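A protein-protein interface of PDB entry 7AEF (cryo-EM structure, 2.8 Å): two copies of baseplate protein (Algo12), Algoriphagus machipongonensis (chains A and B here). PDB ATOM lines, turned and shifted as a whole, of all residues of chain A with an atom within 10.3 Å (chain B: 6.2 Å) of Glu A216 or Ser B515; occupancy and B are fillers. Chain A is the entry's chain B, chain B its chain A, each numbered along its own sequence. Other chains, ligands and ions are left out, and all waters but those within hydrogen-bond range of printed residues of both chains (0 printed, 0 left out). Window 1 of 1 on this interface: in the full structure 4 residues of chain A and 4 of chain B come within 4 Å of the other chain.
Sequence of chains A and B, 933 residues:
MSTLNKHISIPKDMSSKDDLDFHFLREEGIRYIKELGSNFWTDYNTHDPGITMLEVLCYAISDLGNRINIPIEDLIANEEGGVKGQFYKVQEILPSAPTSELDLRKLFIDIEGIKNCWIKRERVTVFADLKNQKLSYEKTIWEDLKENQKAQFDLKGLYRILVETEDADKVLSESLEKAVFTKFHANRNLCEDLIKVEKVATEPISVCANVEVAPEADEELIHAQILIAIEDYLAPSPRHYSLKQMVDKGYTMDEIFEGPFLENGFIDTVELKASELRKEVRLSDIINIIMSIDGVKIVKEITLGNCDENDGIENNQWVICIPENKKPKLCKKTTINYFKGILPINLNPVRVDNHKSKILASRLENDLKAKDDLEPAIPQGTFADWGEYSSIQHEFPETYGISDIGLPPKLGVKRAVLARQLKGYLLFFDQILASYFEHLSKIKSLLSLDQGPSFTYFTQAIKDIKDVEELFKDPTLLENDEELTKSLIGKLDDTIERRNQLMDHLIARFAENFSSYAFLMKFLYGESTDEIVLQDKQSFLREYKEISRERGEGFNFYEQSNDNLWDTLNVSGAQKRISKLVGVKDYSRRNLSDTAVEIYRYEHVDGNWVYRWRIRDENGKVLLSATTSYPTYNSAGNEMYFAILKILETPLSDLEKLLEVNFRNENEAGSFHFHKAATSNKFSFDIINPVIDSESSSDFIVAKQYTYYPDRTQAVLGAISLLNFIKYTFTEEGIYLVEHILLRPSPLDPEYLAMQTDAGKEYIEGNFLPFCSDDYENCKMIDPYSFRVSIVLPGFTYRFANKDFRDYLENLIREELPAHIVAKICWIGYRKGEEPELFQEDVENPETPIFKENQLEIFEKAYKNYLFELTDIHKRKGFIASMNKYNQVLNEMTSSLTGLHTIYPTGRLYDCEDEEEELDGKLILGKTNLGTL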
ATOM      1  N   GLU A 212      16.120 -25.146 -32.857  1.00  0.00           N
ATOM      2  CA  GLU A 212      16.930 -24.932 -31.668  1.00  0.00           C
ATOM      3  C   GLU A 212      17.966 -23.859 -31.937  1.00  0.00           C
ATOM      4  O   GLU A 212      18.665 -23.895 -32.957  1.00  0.00           O
ATOM      5  CB  GLU A 212      17.648 -26.197 -31.217  1.00  0.00           C
ATOM      6  CG  GLU A 212      18.476 -25.964 -29.952  1.00  0.00           C
ATOM      7  CD  GLU A 212      19.083 -27.179 -29.409  1.00  0.00           C
ATOM      8  OE1 GLU A 212      18.833 -28.240 -29.951  1.00  0.00           O
ATOM      9  OE2 GLU A 212      19.889 -27.068 -28.491  1.00  0.00           O
ATOM     10  N   VAL A 213      18.093 -22.936 -30.991  1.00  0.00           N
ATOM     11  CA  VAL A 213      19.012 -21.825 -31.110  1.00  0.00           C
ATOM     12  C   VAL A 213      20.004 -21.831 -29.960  1.00  0.00           C
ATOM     13  O   VAL A 213      19.810 -22.497 -28.949  1.00  0.00           O
ATOM     14  CB  VAL A 213      18.268 -20.483 -31.157  1.00  0.00           C
ATOM     15  CG1 VAL A 213      17.330 -20.449 -32.366  1.00  0.00           C
ATOM     16  CG2 VAL A 213      17.497 -20.265 -29.856  1.00  0.00           C
ATOM     17  N   ALA A 214      21.067 -21.051 -30.133  1.00  0.00           N
ATOM     18  CA  ALA A 214      22.099 -20.905 -29.129  1.00  0.00           C
ATOM     19  C   ALA A 214      21.509 -20.364 -27.824  1.00  0.00           C
ATOM     20  O   ALA A 214      20.585 -19.556 -27.861  1.00  0.00           O
ATOM     21  CB  ALA A 214      23.177 -19.957 -29.651  1.00  0.00           C
ATOM     22  N   PRO A 215      22.057 -20.794 -26.674  1.00  0.00           N
ATOM     23  CA  PRO A 215      21.605 -20.363 -25.333  1.00  0.00           C
ATOM     24  C   PRO A 215      21.740 -18.876 -25.089  1.00  0.00           C
ATOM     25  O   PRO A 215      21.099 -18.326 -24.188  1.00  0.00           O
ATOM     26  CB  PRO A 215      22.540 -21.158 -24.403  1.00  0.00           C
ATOM     27  CG  PRO A 215      23.736 -21.487 -25.246  1.00  0.00           C
ATOM     28  CD  PRO A 215      23.194 -21.717 -26.610  1.00  0.00           C
ATOM     29  N   GLU A 216      22.573 -18.215 -25.864  1.00  0.00           N
ATOM     30  CA  GLU A 216      22.817 -16.781 -25.815  1.00  0.00           C
ATOM     31  C   GLU A 216      22.502 -16.194 -27.160  1.00  0.00           C
ATOM     32  O   GLU A 216      23.397 -15.886 -27.942  1.00  0.00           O
ATOM     33  CB  GLU A 216      24.255 -16.500 -25.383  1.00  0.00           C
ATOM     34  CG  GLU A 216      24.660 -17.104 -24.054  1.00  0.00           C
ATOM     35  CD  GLU A 216      26.046 -16.698 -23.601  1.00  0.00           C
ATOM     36  OE1 GLU A 216      26.789 -16.137 -24.402  1.00  0.00           O
ATOM     37  OE2 GLU A 216      26.427 -17.039 -22.484  1.00  0.00           O
ATOM     38  N   ALA A 217      21.214 -16.024 -27.418  1.00  0.00           N
ATOM     39  CA  ALA A 217      20.747 -15.549 -28.702  1.00  0.00           C
ATOM     40  C   ALA A 217      19.470 -14.756 -28.512  1.00  0.00           C
ATOM     41  O   ALA A 217      18.662 -15.050 -27.630  1.00  0.00           O
ATOM     42  CB  ALA A 217      20.500 -16.707 -29.661  1.00  0.00           C
ATOM     43  N   ASP A 218      19.295 -13.764 -29.375  1.00  0.00           N
ATOM     44  CA  ASP A 218      18.110 -12.908 -29.413  1.00  0.00           C
ATOM     45  C   ASP A 218      17.104 -13.552 -30.357  1.00  0.00           C
ATOM     46  O   ASP A 218      17.250 -13.496 -31.580  1.00  0.00           O
ATOM     47  CB  ASP A 218      18.546 -11.502 -29.832  1.00  0.00           C
ATOM     48  CG  ASP A 218      17.421 -10.482 -29.898  1.00  0.00           C
ATOM     49  OD1 ASP A 218      16.325 -10.796 -30.353  1.00  0.00           O
ATOM     50  OD2 ASP A 218      17.649  -9.337 -29.496  1.00  0.00           O
ATOM     51  N   GLU A 219      16.101 -14.196 -29.768  1.00  0.00           N
ATOM     52  CA  GLU A 219      15.114 -14.937 -30.528  1.00  0.00           C
ATOM     53  C   GLU A 219      14.161 -14.069 -31.329  1.00  0.00           C
ATOM     54  O   GLU A 219      13.742 -14.479 -32.417  1.00  0.00           O
ATOM     55  CB  GLU A 219      14.396 -15.879 -29.612  1.00  0.00           C
ATOM     56  CG  GLU A 219      15.174 -17.002 -29.119  1.00  0.00           C
ATOM     57  CD  GLU A 219      14.478 -17.807 -28.091  1.00  0.00           C
ATOM     58  OE1 GLU A 219      13.753 -17.221 -27.306  1.00  0.00           O
ATOM     59  OE2 GLU A 219      14.642 -19.028 -28.073  1.00  0.00           O
ATOM     60  N   GLU A 220      13.794 -12.900 -30.821  1.00  0.00           N
ATOM     61  CA  GLU A 220      12.888 -12.059 -31.587  1.00  0.00           C
ATOM     62  C   GLU A 220      13.566 -11.611 -32.869  1.00  0.00           C
ATOM     63  O   GLU A 220      12.951 -11.626 -33.941  1.00  0.00           O
ATOM     64  CB  GLU A 220      12.441 -10.867 -30.746  1.00  0.00           C
ATOM     65  CG  GLU A 220      11.619 -11.260 -29.521  1.00  0.00           C
ATOM     66  CD  GLU A 220      12.480 -11.637 -28.349  1.00  0.00           C
ATOM     67  OE1 GLU A 220      13.690 -11.691 -28.513  1.00  0.00           O
ATOM     68  OE2 GLU A 220      11.968 -11.844 -27.261  1.00  0.00           O
ATOM     69  N   LEU A 221      14.864 -11.311 -32.781  1.00  0.00           N
ATOM     70  CA  LEU A 221      15.614 -10.926 -33.964  1.00  0.00           C
ATOM     71  C   LEU A 221      15.778 -12.089 -34.917  1.00  0.00           C
ATOM     72  O   LEU A 221      15.628 -11.899 -36.129  1.00  0.00           O
ATOM     73  CB  LEU A 221      16.977 -10.358 -33.596  1.00  0.00           C
ATOM     74  CG  LEU A 221      17.859  -9.914 -34.774  1.00  0.00           C
ATOM     75  CD1 LEU A 221      17.164  -8.850 -35.637  1.00  0.00           C
ATOM     76  CD2 LEU A 221      19.147  -9.376 -34.227  1.00  0.00           C
ATOM     77  N   ILE A 222      16.069 -13.292 -34.399  1.00  0.00           N
ATOM     78  CA  ILE A 222      16.207 -14.450 -35.277  1.00  0.00           C
ATOM     79  C   ILE A 222      14.923 -14.680 -36.028  1.00  0.00           C
ATOM     80  O   ILE A 222      14.949 -14.917 -37.239  1.00  0.00           O
ATOM     81  CB  ILE A 222      16.612 -15.728 -34.516  1.00  0.00           C
ATOM     82  CG1 ILE A 222      18.056 -15.614 -34.037  1.00  0.00           C
ATOM     83  CG2 ILE A 222      16.412 -16.991 -35.394  1.00  0.00           C
ATOM     84  CD1 ILE A 222      18.491 -16.671 -33.051  1.00  0.00           C
ATOM     85  N   ASP A 294      22.368 -16.628 -38.128  1.00  0.00           N
ATOM     86  CA  ASP A 294      23.227 -16.649 -36.956  1.00  0.00           C
ATOM     87  C   ASP A 294      22.450 -16.912 -35.671  1.00  0.00           C
ATOM     88  O   ASP A 294      21.521 -16.187 -35.330  1.00  0.00           O
ATOM     89  CB  ASP A 294      24.012 -15.355 -36.821  1.00  0.00           C
ATOM     90  CG  ASP A 294      25.123 -15.494 -35.818  1.00  0.00           C
ATOM     91  OD1 ASP A 294      25.183 -16.526 -35.145  1.00  0.00           O
ATOM     92  OD2 ASP A 294      25.914 -14.574 -35.654  1.00  0.00           O
ATOM     93  N   GLY A 295      22.885 -17.948 -34.951  1.00  0.00           N
ATOM     94  CA  GLY A 295      22.265 -18.399 -33.724  1.00  0.00           C
ATOM     95  C   GLY A 295      21.495 -19.691 -33.884  1.00  0.00           C
ATOM     96  O   GLY A 295      21.199 -20.351 -32.888  1.00  0.00           O
ATOM     97  N   VAL A 296      21.172 -20.083 -35.105  1.00  0.00           N
ATOM     98  CA  VAL A 296      20.471 -21.345 -35.321  1.00  0.00           C
ATOM     99  C   VAL A 296      21.430 -22.511 -35.250  1.00  0.00           C
ATOM    100  O   VAL A 296      22.472 -22.507 -35.906  1.00  0.00           O
ATOM    101  CB  VAL A 296      19.715 -21.341 -36.656  1.00  0.00           C
ATOM    102  CG1 VAL A 296      19.065 -22.718 -36.896  1.00  0.00           C
ATOM    103  CG2 VAL A 296      18.616 -20.265 -36.608  1.00  0.00           C
ATOM    104  N   LYS A 297      21.076 -23.519 -34.458  1.00  0.00           N
ATOM    105  CA  LYS A 297      21.913 -24.689 -34.365  1.00  0.00           C
ATOM    106  C   LYS A 297      21.310 -25.906 -35.035  1.00  0.00           C
ATOM    107  O   LYS A 297      22.011 -26.624 -35.763  1.00  0.00           O
ATOM    108  CB  LYS A 297      22.237 -25.022 -32.918  1.00  0.00           C
ATOM    109  CG  LYS A 297      22.943 -23.919 -32.148  1.00  0.00           C
ATOM    110  CD  LYS A 297      24.403 -23.818 -32.604  1.00  0.00           C
ATOM    111  CE  LYS A 297      25.150 -22.726 -31.873  1.00  0.00           C
ATOM    112  NZ  LYS A 297      26.562 -22.611 -32.332  1.00  0.00           N
ATOM    113  N   PHE A 339      13.479 -23.272 -29.438  1.00  0.00           N
ATOM    114  CA  PHE A 339      13.955 -23.986 -28.262  1.00  0.00           C
ATOM    115  C   PHE A 339      15.401 -23.675 -27.896  1.00  0.00           C
ATOM    116  O   PHE A 339      16.247 -23.435 -28.759  1.00  0.00           O
ATOM    117  CB  PHE A 339      13.894 -25.486 -28.476  1.00  0.00           C
ATOM    118  CG  PHE A 339      12.542 -26.005 -28.744  1.00  0.00           C
ATOM    119  CD1 PHE A 339      12.029 -26.012 -30.028  1.00  0.00           C
ATOM    120  CD2 PHE A 339      11.784 -26.520 -27.728  1.00  0.00           C
ATOM    121  CE1 PHE A 339      10.779 -26.493 -30.278  1.00  0.00           C
ATOM    122  CE2 PHE A 339      10.542 -27.015 -27.992  1.00  0.00           C
ATOM    123  CZ  PHE A 339      10.031 -26.992 -29.253  1.00  0.00           C
ATOM    124  N   LYS A 340      15.696 -23.776 -26.605  1.00  0.00           N
ATOM    125  CA  LYS A 340      17.070 -23.745 -26.116  1.00  0.00           C
ATOM    126  C   LYS A 340      17.299 -25.023 -25.328  1.00  0.00           C
ATOM    127  O   LYS A 340      16.709 -25.208 -24.259  1.00  0.00           O
ATOM    128  CB  LYS A 340      17.348 -22.514 -25.254  1.00  0.00           C
ATOM    129  CG  LYS A 340      17.409 -21.202 -26.020  1.00  0.00           C
ATOM    130  CD  LYS A 340      17.623 -20.013 -25.083  1.00  0.00           C
ATOM    131  CE  LYS A 340      17.752 -18.707 -25.849  1.00  0.00           C
ATOM    132  NZ  LYS A 340      17.942 -17.542 -24.942  1.00  0.00           N
ATOM    133  N   GLY A 341      18.176 -25.881 -25.826  1.00  0.00           N
ATOM    134  CA  GLY A 341      18.315 -27.170 -25.186  1.00  0.00           C
ATOM    135  C   GLY A 341      17.003 -27.894 -25.368  1.00  0.00           C
ATOM    136  O   GLY A 341      16.568 -28.149 -26.490  1.00  0.00           O
ATOM    137  N   ILE A 345      10.651 -21.664 -25.839  1.00  0.00           N
ATOM    138  CA  ILE A 345      10.669 -20.283 -25.365  1.00  0.00           C
ATOM    139  C   ILE A 345       9.620 -19.520 -26.160  1.00  0.00           C
ATOM    140  O   ILE A 345       9.268 -19.887 -27.285  1.00  0.00           O
ATOM    141  CB  ILE A 345      12.063 -19.600 -25.466  1.00  0.00           C
ATOM    142  CG1 ILE A 345      13.127 -20.429 -24.788  1.00  0.00           C
ATOM    143  CG2 ILE A 345      12.169 -18.313 -24.651  1.00  0.00           C
ATOM    144  CD1 ILE A 345      13.858 -21.224 -25.722  1.00  0.00           C
ATOM    145  N   ASP B 504      32.675 -12.487 -17.360  1.00  0.00           N
ATOM    146  CA  ASP B 504      32.796 -13.770 -18.023  1.00  0.00           C
ATOM    147  C   ASP B 504      34.244 -14.156 -18.186  1.00  0.00           C
ATOM    148  O   ASP B 504      34.592 -15.322 -17.999  1.00  0.00           O
ATOM    149  CB  ASP B 504      32.104 -13.751 -19.373  1.00  0.00           C
ATOM    150  CG  ASP B 504      30.590 -13.727 -19.254  1.00  0.00           C
ATOM    151  OD1 ASP B 504      30.046 -13.970 -18.172  1.00  0.00           O
ATOM    152  OD2 ASP B 504      29.938 -13.489 -20.261  1.00  0.00           O
ATOM    153  N   ASN B 513      31.458 -21.723 -16.087  1.00  0.00           N
ATOM    154  CA  ASN B 513      30.603 -21.165 -17.153  1.00  0.00           C
ATOM    155  C   ASN B 513      29.163 -20.891 -16.696  1.00  0.00           C
ATOM    156  O   ASN B 513      28.436 -21.813 -16.322  1.00  0.00           O
ATOM    157  CB  ASN B 513      30.622 -22.110 -18.352  1.00  0.00           C
ATOM    158  CG  ASN B 513      29.970 -21.533 -19.596  1.00  0.00           C
ATOM    159  OD1 ASN B 513      28.964 -20.820 -19.564  1.00  0.00           O
ATOM    160  ND2 ASN B 513      30.545 -21.872 -20.729  1.00  0.00           N
ATOM    161  N   PHE B 514      28.731 -19.624 -16.800  1.00  0.00           N
ATOM    162  CA  PHE B 514      27.402 -19.162 -16.384  1.00  0.00           C
ATOM    163  C   PHE B 514      26.428 -18.860 -17.524  1.00  0.00           C
ATOM    164  O   PHE B 514      25.440 -18.151 -17.307  1.00  0.00           O
ATOM    165  CB  PHE B 514      27.531 -17.913 -15.530  1.00  0.00           C
ATOM    166  CG  PHE B 514      27.790 -18.201 -14.135  1.00  0.00           C
ATOM    167  CD1 PHE B 514      26.839 -17.868 -13.218  1.00  0.00           C
ATOM    168  CD2 PHE B 514      28.935 -18.838 -13.722  1.00  0.00           C
ATOM    169  CE1 PHE B 514      27.003 -18.137 -11.914  1.00  0.00           C
ATOM    170  CE2 PHE B 514      29.104 -19.116 -12.410  1.00  0.00           C
ATOM    171  CZ  PHE B 514      28.131 -18.761 -11.500  1.00  0.00           C
ATOM    172  N   SER B 515      26.663 -19.404 -18.710  1.00  0.00           N
ATOM    173  CA  SER B 515      25.790 -19.141 -19.857  1.00  0.00           C
ATOM    174  C   SER B 515      24.303 -19.377 -19.631  1.00  0.00           C
ATOM    175  O   SER B 515      23.475 -18.601 -20.107  1.00  0.00           O
ATOM    176  CB  SER B 515      26.218 -19.958 -21.059  1.00  0.00           C
ATOM    177  OG  SER B 515      27.520 -19.649 -21.465  1.00  0.00           O
ATOM    178  N   SER B 516      23.943 -20.402 -18.869  1.00  0.00           N
ATOM    179  CA  SER B 516      22.533 -20.753 -18.711  1.00  0.00           C
ATOM    180  C   SER B 516      21.710 -19.697 -17.970  1.00  0.00           C
ATOM    181  O   SER B 516      20.482 -19.669 -18.110  1.00  0.00           O
ATOM    182  CB  SER B 516      22.398 -22.050 -17.949  1.00  0.00           C
ATOM    183  OG  SER B 516      22.879 -21.912 -16.637  1.00  0.00           O
ATOM    184  N   TYR B 517      22.347 -18.785 -17.237  1.00  0.00           N
ATOM    185  CA  TYR B 517      21.590 -17.767 -16.520  1.00  0.00           C
ATOM    186  C   TYR B 517      20.903 -16.829 -17.472  1.00  0.00           C
ATOM    187  O   TYR B 517      19.861 -16.258 -17.142  1.00  0.00           O
ATOM    188  CB  TYR B 517      22.503 -16.976 -15.606  1.00  0.00           C
ATOM    189  CG  TYR B 517      22.702 -17.660 -14.335  1.00  0.00           C
ATOM    190  CD1 TYR B 517      23.546 -18.737 -14.249  1.00  0.00           C
ATOM    191  CD2 TYR B 517      22.038 -17.223 -13.213  1.00  0.00           C
ATOM    192  CE1 TYR B 517      23.717 -19.369 -13.066  1.00  0.00           C
ATOM    193  CE2 TYR B 517      22.201 -17.837 -12.027  1.00  0.00           C
ATOM    194  CZ  TYR B 517      23.039 -18.914 -11.950  1.00  0.00           C
ATOM    195  OH  TYR B 517      23.218 -19.554 -10.750  1.00  0.00           O
ATOM    196  N   ALA B 518      21.442 -16.753 -18.678  1.00  0.00           N
ATOM    197  CA  ALA B 518      20.920 -15.897 -19.713  1.00  0.00           C
ATOM    198  C   ALA B 518      19.470 -16.189 -20.019  1.00  0.00           C
ATOM    199  O   ALA B 518      18.740 -15.281 -20.411  1.00  0.00           O
ATOM    200  CB  ALA B 518      21.742 -16.069 -20.979  1.00  0.00           C
ATOM    201  N   PHE B 519      19.028 -17.431 -19.880  1.00  0.00           N
ATOM    202  CA  PHE B 519      17.635 -17.677 -20.153  1.00  0.00           C
ATOM    203  C   PHE B 519      16.898 -18.267 -18.981  1.00  0.00           C
ATOM    204  O   PHE B 519      15.687 -18.076 -18.888  1.00  0.00           O
ATOM    205  CB  PHE B 519      17.474 -18.569 -21.385  1.00  0.00           C
ATOM    206  CG  PHE B 519      17.942 -19.952 -21.196  1.00  0.00           C
ATOM    207  CD1 PHE B 519      17.076 -20.928 -20.766  1.00  0.00           C
ATOM    208  CD2 PHE B 519      19.243 -20.297 -21.472  1.00  0.00           C
ATOM    209  CE1 PHE B 519      17.498 -22.204 -20.600  1.00  0.00           C
ATOM    210  CE2 PHE B 519      19.667 -21.587 -21.306  1.00  0.00           C
ATOM    211  CZ  PHE B 519      18.792 -22.538 -20.867  1.00  0.00           C
ATOM    212  N   LYS B 537      27.059 -13.329 -10.413  1.00  0.00           N
ATOM    213  CA  LYS B 537      28.385 -13.663 -10.917  1.00  0.00           C
ATOM    214  C   LYS B 537      29.478 -13.159  -9.982  1.00  0.00           C
ATOM    215  O   LYS B 537      30.450 -13.879  -9.732  1.00  0.00           O
ATOM    216  CB  LYS B 537      28.586 -13.117 -12.327  1.00  0.00           C
ATOM    217  CG  LYS B 537      27.805 -13.856 -13.400  1.00  0.00           C
ATOM    218  CD  LYS B 537      28.042 -13.282 -14.803  1.00  0.00           C
ATOM    219  CE  LYS B 537      27.229 -14.049 -15.843  1.00  0.00           C
ATOM    220  NZ  LYS B 537      27.401 -13.545 -17.236  1.00  0.00           N
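The backbone carbonyl oxygen (O) of Pro A215 lies within hydrogen-bond range of the side-chain amino group (NZ) of Lys A340 (3.3 Å).
OD1 of Asn B513 is in hydrogen-bond range of OG of Ser B515 (2.7 Å).
The side-chain carboxylate of Glu A216 sits at hydrogen-bond distance from the side-chain hydroxyl of Ser B515.
Among the printed residues, pairs that only touch across the chains: Pro A215 with Ala B518, Pro A215 with Phe B519 and Lys A340 with Phe B519.
No position is printed for both chains.
Of the 4 pairs that touch across the chains among the printed residues, none has its exchanged pair printed and touching as well.
Glu A216 touches just one residue of chain B: Ser B515.
Ser B515 touches one residue of chain A.
No residue of chain A comes within 4 Å of Asn B513.
Printed residues of chain A within 4 Å of Ala B518: Pro A215 (3.98 Å).
Of the printed residues of chain B, Lys A340 touches Phe B519 (3.7 Å).
Of the printed residues of chain A, Phe B519 touches Pro A215 (3.8 Å) and Lys A340 (3.7 Å).
The nearest residue of chain B that does not touch Glu A216 is Ala B518 (4.4 Å).
The nearest printed residue of chain B that does not touch Pro A215 is Ser B515 (4.7 Å).
Printed residues of chain B that touch a printed residue of chain A: Ser B515, Ala B518 and Phe B519.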
